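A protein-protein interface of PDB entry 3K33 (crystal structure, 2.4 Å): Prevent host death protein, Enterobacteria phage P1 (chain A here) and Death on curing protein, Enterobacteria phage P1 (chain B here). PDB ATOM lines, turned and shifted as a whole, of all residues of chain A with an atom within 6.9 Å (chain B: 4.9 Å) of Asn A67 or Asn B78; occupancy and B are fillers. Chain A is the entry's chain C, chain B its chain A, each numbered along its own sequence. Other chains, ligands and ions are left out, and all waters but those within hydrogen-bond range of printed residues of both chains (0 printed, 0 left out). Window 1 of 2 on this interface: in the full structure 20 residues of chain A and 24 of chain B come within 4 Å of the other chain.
The side-chain amide nitrogen of Asn B16 is in hydrogen-bond range of the side-chain amide oxygen of Asn A67, at 2.9 Å.
The backbone carbonyl oxygen of Phe A60 sits at hydrogen-bond distance from the side-chain hydroxyl of Tyr B20 (3.1 Å).
The side-chain hydroxyl of Tyr B20 lies within hydrogen-bond range of the side-chain carboxylate of Asp A64, 2.6 Å away.
ND2 of Asn B78 sits at hydrogen-bond distance from OD1 of Asn A67 (2.7 Å).
The side-chain amino group of Lys A68 is in salt-bridge range of the side-chain carboxylate of Asp A64 (2.7 Å).
The backbone carbonyl oxygen (O) of Leu A63 is in hydrogen-bond range of the side-chain amide nitrogen (ND2) of Asn A67.
The backbone carbonyl oxygen of Arg B74 sits at hydrogen-bond distance from the side-chain amide nitrogen of Asn B78 (3.0 Å).
ND2 of Asn B16 sits close to ND2 of Asn B78 (3.1 Å).
The guanidinium group (NH1) of Arg B74 lies within hydrogen-bond range of the side-chain amide oxygen (OD1) of Asn B16 (2.9 Å).
CD2 of Leu A59 touches O of Asn B78, 3.6 Å away.
O of Leu B12 touches CZ of Phe A60, at 3.5 Å.
Asn B16 touches Phe A60 (N to CE2, 3.6 Å).
CE1 of Phe A60 touches ND2 of Asn B78 (3.7 Å).
Leu B81 touches Leu A63.
CB of Asn A67 touches CZ of Tyr B20, at 3.4 Å.
Asn A67 touches Arg B74 (O to CD, 3.3 Å).
CG of Lys A68 touches CD1 of Tyr B20 (3.8 Å).
Arg B74 touches Leu A70 (CG to CB, 3.8 Å).
CZ of Arg B74 touches CG2 of Val A71, at 3.6 Å.
Of chain B, only Asn B16 (2.9 Å), Tyr B20 (3.4 Å), Arg B74 (3.3 Å) and Asn B78 (2.7 Å) come within 4 Å of Asn A67.
Asn B78 touches just these residues of chain A: Leu A59 (3.6 Å), Phe A60 (3.7 Å), Leu A63 (3.3 Å) and Asn A67 (2.7 Å).
Of the printed residues of chain B, Val A71 touches Arg B74.
Printed residues of chain B within 4 Å of Leu A59: Asn B78 (3.6 Å).
Printed residues of chain A within 4 Å of Tyr B20: Phe A60, Asp A64, Asn A67 and Lys A68.
Printed residues of chain B within 4 Å of Asp A64: Tyr B20 (2.6 Å).
Of the printed residues of chain A, Arg B74 touches Asn A67 (3.3 Å), Leu A70 (3.8 Å) and Val A71 (3.6 Å).
The nearest printed residue of chain B that does not touch Phe A60 is Arg B74 (6.4 Å).
Hydrophobic or aromatic side chains of chain B that line the printed part of chain A: Tyr B20, Leu B77 and Leu B81.
Of the 14 printed residues of chain A, 9 touch a printed residue of chain B.
Among the printed residues, 17 pairs touch across the chains.
Among the printed residues, no Asp or Glu carboxylate lies within 4 Å of a Lys or Arg side-chain nitrogen of the other chain.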
ATOM      1  N   LEU A  59     -22.134  -3.076  35.282  1.00  0.00           N
ATOM      2  CA  LEU A  59     -22.863  -3.493  34.087  1.00  0.00           C
ATOM      3  C   LEU A  59     -22.039  -3.021  32.900  1.00  0.00           C
ATOM      4  O   LEU A  59     -21.736  -3.793  31.985  1.00  0.00           O
ATOM      5  CB  LEU A  59     -24.254  -2.851  34.043  1.00  0.00           C
ATOM      6  CG  LEU A  59     -25.102  -3.099  32.792  1.00  0.00           C
ATOM      7  CD1 LEU A  59     -25.574  -4.552  32.748  1.00  0.00           C
ATOM      8  CD2 LEU A  59     -26.274  -2.148  32.784  1.00  0.00           C
ATOM      9  N   PHE A  60     -21.665  -1.744  32.946  1.00  0.00           N
ATOM     10  CA  PHE A  60     -20.851  -1.126  31.911  1.00  0.00           C
ATOM     11  C   PHE A  60     -19.488  -1.797  31.757  1.00  0.00           C
ATOM     12  O   PHE A  60     -19.012  -1.953  30.636  1.00  0.00           O
ATOM     13  CB  PHE A  60     -20.661   0.364  32.194  1.00  0.00           C
ATOM     14  CG  PHE A  60     -21.940   1.147  32.241  1.00  0.00           C
ATOM     15  CD1 PHE A  60     -23.122   0.621  31.726  1.00  0.00           C
ATOM     16  CD2 PHE A  60     -21.954   2.432  32.776  1.00  0.00           C
ATOM     17  CE1 PHE A  60     -24.305   1.363  31.749  1.00  0.00           C
ATOM     18  CE2 PHE A  60     -23.120   3.184  32.800  1.00  0.00           C
ATOM     19  CZ  PHE A  60     -24.305   2.646  32.284  1.00  0.00           C
ATOM     20  N   ASP A  61     -18.856  -2.175  32.868  1.00  0.00           N
ATOM     21  CA  ASP A  61     -17.585  -2.902  32.800  1.00  0.00           C
ATOM     22  C   ASP A  61     -17.773  -4.139  31.932  1.00  0.00           C
ATOM     23  O   ASP A  61     -17.051  -4.346  30.952  1.00  0.00           O
ATOM     24  CB  ASP A  61     -17.099  -3.356  34.190  1.00  0.00           C
ATOM     25  CG  ASP A  61     -16.603  -2.207  35.054  1.00  0.00           C
ATOM     26  OD1 ASP A  61     -16.147  -1.186  34.502  1.00  0.00           O
ATOM     27  OD2 ASP A  61     -16.639  -2.344  36.298  1.00  0.00           O
ATOM     28  N   THR A  62     -18.767  -4.945  32.304  1.00  0.00           N
ATOM     29  CA  THR A  62     -19.088  -6.196  31.623  1.00  0.00           C
ATOM     30  C   THR A  62     -19.400  -6.019  30.137  1.00  0.00           C
ATOM     31  O   THR A  62     -19.130  -6.905  29.329  1.00  0.00           O
ATOM     32  CB  THR A  62     -20.282  -6.897  32.311  1.00  0.00           C
ATOM     33  OG1 THR A  62     -19.986  -7.079  33.701  1.00  0.00           O
ATOM     34  CG2 THR A  62     -20.565  -8.266  31.677  1.00  0.00           C
ATOM     35  N   LEU A  63     -19.970  -4.878  29.776  1.00  0.00           N
ATOM     36  CA  LEU A  63     -20.347  -4.637  28.389  1.00  0.00           C
ATOM     37  C   LEU A  63     -19.629  -3.418  27.850  1.00  0.00           C
ATOM     38  O   LEU A  63     -20.155  -2.695  27.002  1.00  0.00           O
ATOM     39  CB  LEU A  63     -21.862  -4.449  28.286  1.00  0.00           C
ATOM     40  CG  LEU A  63     -22.731  -5.530  28.934  1.00  0.00           C
ATOM     41  CD1 LEU A  63     -24.195  -5.115  28.851  1.00  0.00           C
ATOM     42  CD2 LEU A  63     -22.497  -6.881  28.252  1.00  0.00           C
ATOM     43  N   ASP A  64     -18.409  -3.201  28.332  1.00  0.00           N
ATOM     44  CA  ASP A  64     -17.631  -2.047  27.923  1.00  0.00           C
ATOM     45  C   ASP A  64     -17.363  -2.051  26.424  1.00  0.00           C
ATOM     46  O   ASP A  64     -17.514  -1.021  25.755  1.00  0.00           O
ATOM     47  CB  ASP A  64     -16.313  -1.990  28.688  1.00  0.00           C
ATOM     48  CG  ASP A  64     -15.692  -0.610  28.660  1.00  0.00           C
ATOM     49  OD1 ASP A  64     -16.344   0.350  29.126  1.00  0.00           O
ATOM     50  OD2 ASP A  64     -14.556  -0.484  28.173  1.00  0.00           O
ATOM     51  N   SER A  65     -16.983  -3.212  25.901  1.00  0.00           N
ATOM     52  CA  SER A  65     -16.647  -3.350  24.482  1.00  0.00           C
ATOM     53  C   SER A  65     -17.832  -2.967  23.580  1.00  0.00           C
ATOM     54  O   SER A  65     -17.724  -2.086  22.727  1.00  0.00           O
ATOM     55  CB  SER A  65     -16.173  -4.784  24.200  1.00  0.00           C
ATOM     56  OG  SER A  65     -15.785  -4.937  22.853  1.00  0.00           O
ATOM     57  N   THR A  66     -18.969  -3.615  23.795  1.00  0.00           N
ATOM     58  CA  THR A  66     -20.162  -3.335  23.008  1.00  0.00           C
ATOM     59  C   THR A  66     -20.656  -1.906  23.225  1.00  0.00           C
ATOM     60  O   THR A  66     -21.043  -1.227  22.268  1.00  0.00           O
ATOM     61  CB  THR A  66     -21.258  -4.344  23.336  1.00  0.00           C
ATOM     62  OG1 THR A  66     -20.753  -5.668  23.098  1.00  0.00           O
ATOM     63  CG2 THR A  66     -22.479  -4.105  22.476  1.00  0.00           C
ATOM     64  N   ASN A  67     -20.632  -1.439  24.475  1.00  0.00           N
ATOM     65  CA  ASN A  67     -21.022  -0.061  24.746  1.00  0.00           C
ATOM     66  C   ASN A  67     -20.214   0.917  23.877  1.00  0.00           C
ATOM     67  O   ASN A  67     -20.775   1.832  23.284  1.00  0.00           O
ATOM     68  CB  ASN A  67     -20.882   0.256  26.240  1.00  0.00           C
ATOM     69  CG  ASN A  67     -22.098  -0.183  27.049  1.00  0.00           C
ATOM     70  OD1 ASN A  67     -23.147   0.444  26.990  1.00  0.00           O
ATOM     71  ND2 ASN A  67     -21.952  -1.255  27.812  1.00  0.00           N
ATOM     72  N   LYS A  68     -18.905   0.707  23.778  1.00  0.00           N
ATOM     73  CA  LYS A  68     -18.085   1.575  22.937  1.00  0.00           C
ATOM     74  C   LYS A  68     -18.311   1.367  21.434  1.00  0.00           C
ATOM     75  O   LYS A  68     -18.274   2.327  20.670  1.00  0.00           O
ATOM     76  CB  LYS A  68     -16.602   1.458  23.301  1.00  0.00           C
ATOM     77  CG  LYS A  68     -16.186   2.478  24.351  1.00  0.00           C
ATOM     78  CD  LYS A  68     -14.740   2.340  24.801  1.00  0.00           C
ATOM     79  CE  LYS A  68     -14.535   1.103  25.662  1.00  0.00           C
ATOM     80  NZ  LYS A  68     -13.318   1.234  26.509  1.00  0.00           N
ATOM     81  N   GLU A  69     -18.559   0.129  21.009  1.00  0.00           N
ATOM     82  CA  GLU A  69     -18.876  -0.106  19.604  1.00  0.00           C
ATOM     83  C   GLU A  69     -20.185   0.581  19.228  1.00  0.00           C
ATOM     84  O   GLU A  69     -20.235   1.343  18.258  1.00  0.00           O
ATOM     85  CB  GLU A  69     -18.977  -1.597  19.269  1.00  0.00           C
ATOM     86  CG  GLU A  69     -19.106  -1.828  17.757  1.00  0.00           C
ATOM     87  CD  GLU A  69     -19.264  -3.280  17.383  1.00  0.00           C
ATOM     88  OE1 GLU A  69     -18.663  -4.143  18.068  1.00  0.00           O
ATOM     89  OE2 GLU A  69     -19.980  -3.561  16.393  1.00  0.00           O
ATOM     90  N   LEU A  70     -21.237   0.319  20.007  1.00  0.00           N
ATOM     91  CA  LEU A  70     -22.560   0.888  19.723  1.00  0.00           C
ATOM     92  C   LEU A  70     -22.561   2.407  19.548  1.00  0.00           C
ATOM     93  O   LEU A  70     -23.454   2.957  18.899  1.00  0.00           O
ATOM     94  CB  LEU A  70     -23.587   0.471  20.792  1.00  0.00           C
ATOM     95  CG  LEU A  70     -24.084  -0.980  20.740  1.00  0.00           C
ATOM     96  CD1 LEU A  70     -25.061  -1.194  21.859  1.00  0.00           C
ATOM     97  CD2 LEU A  70     -24.765  -1.291  19.396  1.00  0.00           C
ATOM     98  N   VAL A  71     -21.572   3.090  20.112  1.00  0.00           N
ATOM     99  CA  VAL A  71     -21.487   4.539  19.926  1.00  0.00           C
ATOM    100  C   VAL A  71     -21.371   4.832  18.421  1.00  0.00           C
ATOM    101  O   VAL A  71     -21.927   5.812  17.908  1.00  0.00           O
ATOM    102  CB  VAL A  71     -20.281   5.139  20.703  1.00  0.00           C
ATOM    103  CG1 VAL A  71     -20.031   6.596  20.285  1.00  0.00           C
ATOM    104  CG2 VAL A  71     -20.544   5.074  22.195  1.00  0.00           C
ATOM    105  N   ASN A  72     -20.669   3.946  17.718  1.00  0.00           N
ATOM    106  CA  ASN A  72     -20.437   4.108  16.293  1.00  0.00           C
ATOM    107  C   ASN A  72     -21.264   3.151  15.435  1.00  0.00           C
ATOM    108  O   ASN A  72     -20.827   2.720  14.366  1.00  0.00           O
ATOM    109  CB  ASN A  72     -18.933   3.974  15.999  1.00  0.00           C
ATOM    110  CG  ASN A  72     -18.126   5.065  16.657  1.00  0.00           C
ATOM    111  OD1 ASN A  72     -17.373   4.822  17.604  1.00  0.00           O
ATOM    112  ND2 ASN A  72     -18.311   6.289  16.188  1.00  0.00           N
ATOM    113  N   LEU B  12     -29.805   4.889  34.202  1.00  0.00           N
ATOM    114  CA  LEU B  12     -28.919   3.980  33.475  1.00  0.00           C
ATOM    115  C   LEU B  12     -28.373   4.696  32.237  1.00  0.00           C
ATOM    116  O   LEU B  12     -27.212   4.529  31.864  1.00  0.00           O
ATOM    117  CB  LEU B  12     -29.691   2.720  33.068  1.00  0.00           C
ATOM    118  CG  LEU B  12     -28.976   1.504  32.472  1.00  0.00           C
ATOM    119  CD1 LEU B  12     -30.009   0.416  32.261  1.00  0.00           C
ATOM    120  CD2 LEU B  12     -28.284   1.832  31.155  1.00  0.00           C
ATOM    121  N   ASN B  16     -24.476   6.238  31.379  1.00  0.00           N
ATOM    122  CA  ASN B  16     -23.884   5.798  30.118  1.00  0.00           C
ATOM    123  C   ASN B  16     -23.518   7.008  29.269  1.00  0.00           C
ATOM    124  O   ASN B  16     -22.472   7.034  28.643  1.00  0.00           O
ATOM    125  CB  ASN B  16     -24.852   4.859  29.379  1.00  0.00           C
ATOM    126  CG  ASN B  16     -24.209   4.154  28.184  1.00  0.00           C
ATOM    127  OD1 ASN B  16     -24.078   4.723  27.100  1.00  0.00           O
ATOM    128  ND2 ASN B  16     -23.812   2.910  28.383  1.00  0.00           N
ATOM    129  N   TYR B  20     -19.601   7.211  28.376  1.00  0.00           N
ATOM    130  CA  TYR B  20     -19.280   6.861  26.998  1.00  0.00           C
ATOM    131  C   TYR B  20     -19.522   8.012  26.041  1.00  0.00           C
ATOM    132  O   TYR B  20     -19.044   7.997  24.899  1.00  0.00           O
ATOM    133  CB  TYR B  20     -20.106   5.652  26.571  1.00  0.00           C
ATOM    134  CG  TYR B  20     -19.783   4.372  27.308  1.00  0.00           C
ATOM    135  CD1 TYR B  20     -18.618   3.648  27.014  1.00  0.00           C
ATOM    136  CD2 TYR B  20     -20.657   3.868  28.286  1.00  0.00           C
ATOM    137  CE1 TYR B  20     -18.323   2.452  27.684  1.00  0.00           C
ATOM    138  CE2 TYR B  20     -20.377   2.682  28.962  1.00  0.00           C
ATOM    139  CZ  TYR B  20     -19.203   1.975  28.658  1.00  0.00           C
ATOM    140  OH  TYR B  20     -18.914   0.800  29.321  1.00  0.00           O
ATOM    141  N   ARG B  74     -27.481   1.923  23.237  1.00  0.00           N
ATOM    142  CA  ARG B  74     -26.728   1.500  24.419  1.00  0.00           C
ATOM    143  C   ARG B  74     -27.651   1.249  25.619  1.00  0.00           C
ATOM    144  O   ARG B  74     -27.541   0.226  26.296  1.00  0.00           O
ATOM    145  CB  ARG B  74     -25.653   2.532  24.784  1.00  0.00           C
ATOM    146  CG  ARG B  74     -24.336   2.391  24.026  1.00  0.00           C
ATOM    147  CD  ARG B  74     -23.422   3.582  24.299  1.00  0.00           C
ATOM    148  NE  ARG B  74     -23.867   4.781  23.587  1.00  0.00           N
ATOM    149  CZ  ARG B  74     -23.538   6.025  23.924  1.00  0.00           C
ATOM    150  NH1 ARG B  74     -22.759   6.256  24.973  1.00  0.00           N
ATOM    151  NH2 ARG B  74     -23.974   7.046  23.201  1.00  0.00           N
ATOM    152  N   THR B  75     -28.568   2.176  25.882  1.00  0.00           N
ATOM    153  CA  THR B  75     -29.522   1.999  26.986  1.00  0.00           C
ATOM    154  C   THR B  75     -30.429   0.765  26.808  1.00  0.00           C
ATOM    155  O   THR B  75     -30.816   0.124  27.797  1.00  0.00           O
ATOM    156  CB  THR B  75     -30.361   3.271  27.176  1.00  0.00           C
ATOM    157  OG1 THR B  75     -29.475   4.382  27.401  1.00  0.00           O
ATOM    158  CG2 THR B  75     -31.300   3.125  28.363  1.00  0.00           C
ATOM    159  N   ALA B  76     -30.755   0.437  25.556  1.00  0.00           N
ATOM    160  CA  ALA B  76     -31.583  -0.740  25.229  1.00  0.00           C
ATOM    161  C   ALA B  76     -30.878  -2.033  25.595  1.00  0.00           C
ATOM    162  O   ALA B  76     -31.435  -2.876  26.290  1.00  0.00           O
ATOM    163  CB  ALA B  76     -31.920  -0.759  23.736  1.00  0.00           C
ATOM    164  N   LEU B  77     -29.653  -2.195  25.109  1.00  0.00           N
ATOM    165  CA  LEU B  77     -28.882  -3.395  25.406  1.00  0.00           C
ATOM    166  C   LEU B  77     -28.587  -3.514  26.910  1.00  0.00           C
ATOM    167  O   LEU B  77     -28.700  -4.595  27.492  1.00  0.00           O
ATOM    168  CB  LEU B  77     -27.565  -3.398  24.622  1.00  0.00           C
ATOM    169  CG  LEU B  77     -26.629  -4.588  24.900  1.00  0.00           C
ATOM    170  CD1 LEU B  77     -27.238  -5.895  24.378  1.00  0.00           C
ATOM    171  CD2 LEU B  77     -25.254  -4.338  24.289  1.00  0.00           C
ATOM    172  N   ASN B  78     -28.187  -2.410  27.533  1.00  0.00           N
ATOM    173  CA  ASN B  78     -27.875  -2.430  28.962  1.00  0.00           C
ATOM    174  C   ASN B  78     -29.098  -2.694  29.837  1.00  0.00           C
ATOM    175  O   ASN B  78     -29.022  -3.463  30.790  1.00  0.00           O
ATOM    176  CB  ASN B  78     -27.171  -1.136  29.384  1.00  0.00           C
ATOM    177  CG  ASN B  78     -25.802  -0.967  28.723  1.00  0.00           C
ATOM    178  OD1 ASN B  78     -25.080  -1.936  28.502  1.00  0.00           O
ATOM    179  ND2 ASN B  78     -25.435   0.273  28.435  1.00  0.00           N
ATOM    180  N   SER B  79     -30.232  -2.079  29.513  1.00  0.00           N
ATOM    181  CA  SER B  79     -31.442  -2.309  30.304  1.00  0.00           C
ATOM    182  C   SER B  79     -31.930  -3.749  30.171  1.00  0.00           C
ATOM    183  O   SER B  79     -32.377  -4.353  31.143  1.00  0.00           O
ATOM    184  CB  SER B  79     -32.538  -1.319  29.910  1.00  0.00           C
ATOM    185  OG  SER B  79     -32.772  -1.338  28.515  1.00  0.00           O
ATOM    186  N   ALA B  80     -31.835  -4.295  28.959  1.00  0.00           N
ATOM    187  CA  ALA B  80     -32.235  -5.672  28.688  1.00  0.00           C
ATOM    188  C   ALA B  80     -31.398  -6.698  29.464  1.00  0.00           C
ATOM    189  O   ALA B  80     -31.938  -7.687  29.955  1.00  0.00           O
ATOM    190  CB  ALA B  80     -32.149  -5.952  27.205  1.00  0.00           C
ATOM    191  N   LEU B  81     -30.085  -6.473  29.554  1.00  0.00           N
ATOM    192  CA  LEU B  81     -29.199  -7.402  30.259  1.00  0.00           C
ATOM    193  C   LEU B  81     -29.182  -7.144  31.762  1.00  0.00           C
ATOM    194  O   LEU B  81     -29.009  -8.070  32.555  1.00  0.00           O
ATOM    195  CB  LEU B  81     -27.779  -7.382  29.672  1.00  0.00           C
ATOM    196  CG  LEU B  81     -27.483  -8.329  28.489  1.00  0.00           C
ATOM    197  CD1 LEU B  81     -28.271  -7.973  27.219  1.00  0.00           C
ATOM    198  CD2 LEU B  81     -25.998  -8.341  28.181  1.00  0.00           C
ATOM    199  N   LEU B  82     -29.372  -5.887  32.152  1.00  0.00           N
ATOM    200  CA  LEU B  82     -29.519  -5.557  33.561  1.00  0.00           C
ATOM    201  C   LEU B  82     -30.762  -6.260  34.096  1.00  0.00           C
ATOM    202  O   LEU B  82     -30.791  -6.682  35.255  1.00  0.00           O
ATOM    203  CB  LEU B  82     -29.672  -4.051  33.767  1.00  0.00           C
ATOM    204  CG  LEU B  82     -29.957  -3.678  35.225  1.00  0.00           C
ATOM    205  CD1 LEU B  82     -28.727  -3.968  36.085  1.00  0.00           C
ATOM    206  CD2 LEU B  82     -30.397  -2.229  35.353  1.00  0.00           C
ATOM    207  N   PHE B  83     -31.791  -6.359  33.251  1.00  0.00           N
ATOM    208  CA  PHE B  83     -33.021  -7.057  33.605  1.00  0.00           C
ATOM    209  C   PHE B  83     -32.753  -8.525  33.927  1.00  0.00           C
ATOM    210  O   PHE B  83     -33.256  -9.049  34.917  1.00  0.00           O
ATOM    211  CB  PHE B  83     -34.040  -6.983  32.468  1.00  0.00           C
ATOM    212  CG  PHE B  83     -35.267  -7.820  32.704  1.00  0.00           C
ATOM    213  CD1 PHE B  83     -36.301  -7.355  33.506  1.00  0.00           C
ATOM    214  CD2 PHE B  83     -35.369  -9.086  32.143  1.00  0.00           C
ATOM    215  CE1 PHE B  83     -37.419  -8.142  33.745  1.00  0.00           C
ATOM    216  CE2 PHE B  83     -36.482  -9.886  32.383  1.00  0.00           C
ATOM    217  CZ  PHE B  83     -37.508  -9.409  33.185  1.00  0.00           C
